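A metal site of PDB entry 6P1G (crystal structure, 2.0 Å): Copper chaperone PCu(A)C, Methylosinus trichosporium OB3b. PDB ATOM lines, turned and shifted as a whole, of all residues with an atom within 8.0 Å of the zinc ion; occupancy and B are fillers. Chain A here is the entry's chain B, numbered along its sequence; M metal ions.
The backbone carbonyl oxygen of Gln 55 lies within hydrogen-bond range of the backbone NH of Glu 87, at 2.7 Å.
OE2 of Glu 87 is in hydrogen-bond range of NE2 of Gln 28 (3.0 Å).
A ring nitrogen (NE2) of His 57 lies within hydrogen-bond range of the side-chain amide oxygen of Gln 55, 3.2 Å away.
A ring nitrogen (ND1) of His 85 sits at hydrogen-bond distance from the backbone carbonyl oxygen (O) of Gly 83, at 3.0 Å.
Of the 18 residues printed, 3 come within 4 Å of the zinc ion.
The zinc ion is bound by a ring nitrogen (NE2) of His 85 (2.0 Å), a ring nitrogen (ND1) of His 57 (2.2 Å) and the side-chain carboxylate (OE1) of Glu 87 (2.6 Å).
The zinc ion has three donor atoms within binding distance.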
ATOM      1  N   ARG A  26     -18.565  17.633 -31.597  1.00  0.00           N
ATOM      2  CA  ARG A  26     -19.360  17.875 -30.402  1.00  0.00           C
ATOM      3  C   ARG A  26     -18.973  16.960 -29.250  1.00  0.00           C
ATOM      4  O   ARG A  26     -18.713  15.772 -29.437  1.00  0.00           O
ATOM      5  CB  ARG A  26     -20.847  17.732 -30.714  1.00  0.00           C
ATOM      6  CG  ARG A  26     -21.368  18.772 -31.684  1.00  0.00           C
ATOM      7  CD  ARG A  26     -22.879  18.778 -31.746  1.00  0.00           C
ATOM      8  NE  ARG A  26     -23.373  19.976 -32.427  1.00  0.00           N
ATOM      9  CZ  ARG A  26     -24.472  20.635 -32.076  1.00  0.00           C
ATOM     10  NH1 ARG A  26     -25.187  20.233 -31.042  1.00  0.00           N
ATOM     11  NH2 ARG A  26     -24.840  21.715 -32.758  1.00  0.00           N
ATOM     12  N   ALA A  27     -18.959  17.525 -28.044  1.00  0.00           N
ATOM     13  CA  ALA A  27     -18.761  16.749 -26.831  1.00  0.00           C
ATOM     14  C   ALA A  27     -19.671  17.273 -25.731  1.00  0.00           C
ATOM     15  O   ALA A  27     -20.301  18.327 -25.878  1.00  0.00           O
ATOM     16  CB  ALA A  27     -17.305  16.792 -26.380  1.00  0.00           C
ATOM     17  N   GLN A  28     -19.741  16.535 -24.628  1.00  0.00           N
ATOM     18  CA  GLN A  28     -20.591  16.915 -23.507  1.00  0.00           C
ATOM     19  C   GLN A  28     -19.735  17.133 -22.276  1.00  0.00           C
ATOM     20  O   GLN A  28     -18.924  16.279 -21.910  1.00  0.00           O
ATOM     21  CB  GLN A  28     -21.660  15.851 -23.243  1.00  0.00           C
ATOM     22  CG  GLN A  28     -22.643  15.643 -24.391  1.00  0.00           C
ATOM     23  CD  GLN A  28     -22.039  14.855 -25.537  1.00  0.00           C
ATOM     24  OE1 GLN A  28     -21.353  13.842 -25.327  1.00  0.00           O
ATOM     25  NE2 GLN A  28     -22.282  15.316 -26.761  1.00  0.00           N
ATOM     26  N   LEU A  29     -19.932  18.278 -21.639  1.00  0.00           N
ATOM     27  CA  LEU A  29     -19.177  18.626 -20.443  1.00  0.00           C
ATOM     28  C   LEU A  29     -20.017  18.331 -19.206  1.00  0.00           C
ATOM     29  O   LEU A  29     -21.162  18.767 -19.095  1.00  0.00           O
ATOM     30  CB  LEU A  29     -18.770  20.099 -20.487  1.00  0.00           C
ATOM     31  CG  LEU A  29     -18.182  20.711 -19.220  1.00  0.00           C
ATOM     32  CD1 LEU A  29     -16.880  20.021 -18.824  1.00  0.00           C
ATOM     33  CD2 LEU A  29     -17.971  22.203 -19.406  1.00  0.00           C
ATOM     34  N   TYR A  30     -19.430  17.579 -18.278  1.00  0.00           N
ATOM     35  CA  TYR A  30     -20.115  17.205 -17.057  1.00  0.00           C
ATOM     36  C   TYR A  30     -19.353  17.724 -15.845  1.00  0.00           C
ATOM     37  O   TYR A  30     -18.140  17.899 -15.905  1.00  0.00           O
ATOM     38  CB  TYR A  30     -20.269  15.688 -16.960  1.00  0.00           C
ATOM     39  CG  TYR A  30     -20.889  15.027 -18.171  1.00  0.00           C
ATOM     40  CD1 TYR A  30     -22.235  15.204 -18.476  1.00  0.00           C
ATOM     41  CD2 TYR A  30     -20.139  14.199 -18.991  1.00  0.00           C
ATOM     42  CE1 TYR A  30     -22.804  14.589 -19.570  1.00  0.00           C
ATOM     43  CE2 TYR A  30     -20.706  13.576 -20.092  1.00  0.00           C
ATOM     44  CZ  TYR A  30     -22.037  13.777 -20.373  1.00  0.00           C
ATOM     45  OH  TYR A  30     -22.607  13.162 -21.467  1.00  0.00           O
ATOM     46  N   GLN A  55     -23.979  25.061 -25.819  1.00  0.00           N
ATOM     47  CA  GLN A  55     -25.400  25.079 -25.538  1.00  0.00           C
ATOM     48  C   GLN A  55     -25.614  24.398 -24.201  1.00  0.00           C
ATOM     49  O   GLN A  55     -24.823  23.544 -23.798  1.00  0.00           O
ATOM     50  CB  GLN A  55     -26.182  24.361 -26.653  1.00  0.00           C
ATOM     51  CG  GLN A  55     -26.032  25.026 -28.009  1.00  0.00           C
ATOM     52  CD  GLN A  55     -26.502  24.129 -29.147  1.00  0.00           C
ATOM     53  OE1 GLN A  55     -26.956  23.003 -28.918  1.00  0.00           O
ATOM     54  NE2 GLN A  55     -26.407  24.634 -30.369  1.00  0.00           N
ATOM     55  N   PHE A  56     -26.665  24.793 -23.485  1.00  0.00           N
ATOM     56  CA  PHE A  56     -26.984  24.166 -22.208  1.00  0.00           C
ATOM     57  C   PHE A  56     -28.165  23.235 -22.415  1.00  0.00           C
ATOM     58  O   PHE A  56     -29.226  23.666 -22.849  1.00  0.00           O
ATOM     59  CB  PHE A  56     -27.299  25.224 -21.149  1.00  0.00           C
ATOM     60  CG  PHE A  56     -26.144  26.121 -20.826  1.00  0.00           C
ATOM     61  CD1 PHE A  56     -26.310  27.501 -20.808  1.00  0.00           C
ATOM     62  CD2 PHE A  56     -24.899  25.596 -20.530  1.00  0.00           C
ATOM     63  CE1 PHE A  56     -25.248  28.338 -20.512  1.00  0.00           C
ATOM     64  CE2 PHE A  56     -23.835  26.426 -20.241  1.00  0.00           C
ATOM     65  CZ  PHE A  56     -24.003  27.792 -20.224  1.00  0.00           C
ATOM     66  N   HIS A  57     -27.973  21.960 -22.104  1.00  0.00           N
ATOM     67  CA  HIS A  57     -29.039  20.996 -22.343  1.00  0.00           C
ATOM     68  C   HIS A  57     -29.601  20.553 -20.996  1.00  0.00           C
ATOM     69  O   HIS A  57     -28.843  20.246 -20.078  1.00  0.00           O
ATOM     70  CB  HIS A  57     -28.509  19.802 -23.134  1.00  0.00           C
ATOM     71  CG  HIS A  57     -28.156  20.125 -24.556  1.00  0.00           C
ATOM     72  ND1 HIS A  57     -27.657  19.190 -25.433  1.00  0.00           N
ATOM     73  CD2 HIS A  57     -28.222  21.286 -25.240  1.00  0.00           C
ATOM     74  CE1 HIS A  57     -27.437  19.754 -26.602  1.00  0.00           C
ATOM     75  NE2 HIS A  57     -27.772  21.029 -26.515  1.00  0.00           N
ATOM     76  N   ILE A  58     -30.922  20.517 -20.893  1.00  0.00           N
ATOM     77  CA  ILE A  58     -31.597  20.007 -19.705  1.00  0.00           C
ATOM     78  C   ILE A  58     -32.175  18.611 -19.929  1.00  0.00           C
ATOM     79  O   ILE A  58     -32.683  18.307 -21.003  1.00  0.00           O
ATOM     80  CB  ILE A  58     -32.725  20.967 -19.262  1.00  0.00           C
ATOM     81  CG1 ILE A  58     -32.173  22.387 -19.085  1.00  0.00           C
ATOM     82  CG2 ILE A  58     -33.386  20.497 -17.978  1.00  0.00           C
ATOM     83  CD1 ILE A  58     -31.063  22.495 -18.059  1.00  0.00           C
ATOM     84  N   ALA A  59     -32.091  17.771 -18.893  1.00  0.00           N
ATOM     85  CA  ALA A  59     -32.606  16.397 -18.928  1.00  0.00           C
ATOM     86  C   ALA A  59     -32.080  15.607 -20.125  1.00  0.00           C
ATOM     87  O   ALA A  59     -32.708  14.651 -20.573  1.00  0.00           O
ATOM     88  CB  ALA A  59     -34.137  16.403 -18.936  1.00  0.00           C
ATOM     89  N   ALA A  64     -35.173  21.575 -25.563  1.00  0.00           N
ATOM     90  CA  ALA A  64     -34.529  21.084 -24.356  1.00  0.00           C
ATOM     91  C   ALA A  64     -33.265  21.866 -24.027  1.00  0.00           C
ATOM     92  O   ALA A  64     -32.332  21.337 -23.428  1.00  0.00           O
ATOM     93  CB  ALA A  64     -34.219  19.601 -24.486  1.00  0.00           C
ATOM     94  N   ARG A  65     -33.233  23.131 -24.447  1.00  0.00           N
ATOM     95  CA  ARG A  65     -32.077  23.991 -24.204  1.00  0.00           C
ATOM     96  C   ARG A  65     -32.409  25.158 -23.278  1.00  0.00           C
ATOM     97  O   ARG A  65     -33.569  25.519 -23.109  1.00  0.00           O
ATOM     98  CB  ARG A  65     -31.505  24.516 -25.515  1.00  0.00           C
ATOM     99  CG  ARG A  65     -31.328  23.464 -26.596  1.00  0.00           C
ATOM    100  CD  ARG A  65     -30.694  24.079 -27.834  1.00  0.00           C
ATOM    101  NE  ARG A  65     -30.284  23.082 -28.808  1.00  0.00           N
ATOM    102  CZ  ARG A  65     -29.803  23.377 -30.012  1.00  0.00           C
ATOM    103  NH1 ARG A  65     -29.693  24.639 -30.405  1.00  0.00           N
ATOM    104  NH2 ARG A  65     -29.444  22.399 -30.846  1.00  0.00           N
ATOM    105  N   GLY A  83     -28.356  13.148 -17.760  1.00  0.00           N
ATOM    106  CA  GLY A  83     -28.908  14.322 -17.104  1.00  0.00           C
ATOM    107  C   GLY A  83     -28.529  15.597 -17.824  1.00  0.00           C
ATOM    108  O   GLY A  83     -28.179  15.569 -19.014  1.00  0.00           O
ATOM    109  N   SER A  84     -28.601  16.720 -17.124  1.00  0.00           N
ATOM    110  CA  SER A  84     -28.223  18.000 -17.715  1.00  0.00           C
ATOM    111  C   SER A  84     -26.732  18.035 -18.014  1.00  0.00           C
ATOM    112  O   SER A  84     -25.953  17.330 -17.385  1.00  0.00           O
ATOM    113  CB  SER A  84     -28.602  19.152 -16.774  1.00  0.00           C
ATOM    114  OG  SER A  84     -30.006  19.300 -16.697  1.00  0.00           O
ATOM    115  N   HIS A  85     -26.351  18.849 -18.992  1.00  0.00           N
ATOM    116  CA  HIS A  85     -24.948  18.972 -19.367  1.00  0.00           C
ATOM    117  C   HIS A  85     -24.711  20.201 -20.247  1.00  0.00           C
ATOM    118  O   HIS A  85     -25.641  20.797 -20.781  1.00  0.00           O
ATOM    119  CB  HIS A  85     -24.468  17.717 -20.095  1.00  0.00           C
ATOM    120  CG  HIS A  85     -25.290  17.367 -21.296  1.00  0.00           C
ATOM    121  ND1 HIS A  85     -26.451  16.611 -21.219  1.00  0.00           N
ATOM    122  CD2 HIS A  85     -25.134  17.667 -22.608  1.00  0.00           C
ATOM    123  CE1 HIS A  85     -26.962  16.463 -22.428  1.00  0.00           C
ATOM    124  NE2 HIS A  85     -26.186  17.099 -23.286  1.00  0.00           N
ATOM    125  N   VAL A  86     -23.449  20.561 -20.381  1.00  0.00           N
ATOM    126  CA  VAL A  86     -23.056  21.601 -21.324  1.00  0.00           C
ATOM    127  C   VAL A  86     -22.626  20.917 -22.619  1.00  0.00           C
ATOM    128  O   VAL A  86     -21.764  20.032 -22.604  1.00  0.00           O
ATOM    129  CB  VAL A  86     -21.918  22.474 -20.775  1.00  0.00           C
ATOM    130  CG1 VAL A  86     -21.452  23.480 -21.823  1.00  0.00           C
ATOM    131  CG2 VAL A  86     -22.356  23.176 -19.502  1.00  0.00           C
ATOM    132  N   GLU A  87     -23.228  21.326 -23.727  1.00  0.00           N
ATOM    133  CA  GLU A  87     -22.833  20.801 -25.036  1.00  0.00           C
ATOM    134  C   GLU A  87     -21.724  21.683 -25.614  1.00  0.00           C
ATOM    135  O   GLU A  87     -21.895  22.883 -25.766  1.00  0.00           O
ATOM    136  CB  GLU A  87     -24.029  20.774 -25.982  1.00  0.00           C
ATOM    137  CG  GLU A  87     -23.819  19.971 -27.268  1.00  0.00           C
ATOM    138  CD  GLU A  87     -23.999  18.479 -27.073  1.00  0.00           C
ATOM    139  OE1 GLU A  87     -24.564  18.078 -26.035  1.00  0.00           O
ATOM    140  OE2 GLU A  87     -23.612  17.705 -27.976  1.00  0.00           O
ATOM    141  N   LEU A  88     -20.579  21.074 -25.901  1.00  0.00           N
ATOM    142  CA  LEU A  88     -19.471  21.808 -26.517  1.00  0.00           C
ATOM    143  C   LEU A  88     -19.579  21.704 -28.028  1.00  0.00           C
ATOM    144  O   LEU A  88     -19.494  20.611 -28.591  1.00  0.00           O
ATOM    145  CB  LEU A  88     -18.120  21.274 -26.017  1.00  0.00           C
ATOM    146  CG  LEU A  88     -17.968  21.130 -24.501  1.00  0.00           C
ATOM    147  CD1 LEU A  88     -16.582  20.623 -24.135  1.00  0.00           C
ATOM    148  CD2 LEU A  88     -18.262  22.452 -23.783  1.00  0.00           C
HETATM  149 ZN    ZN M   1     -26.821  17.202 -25.209  1.00  0.00          ZN
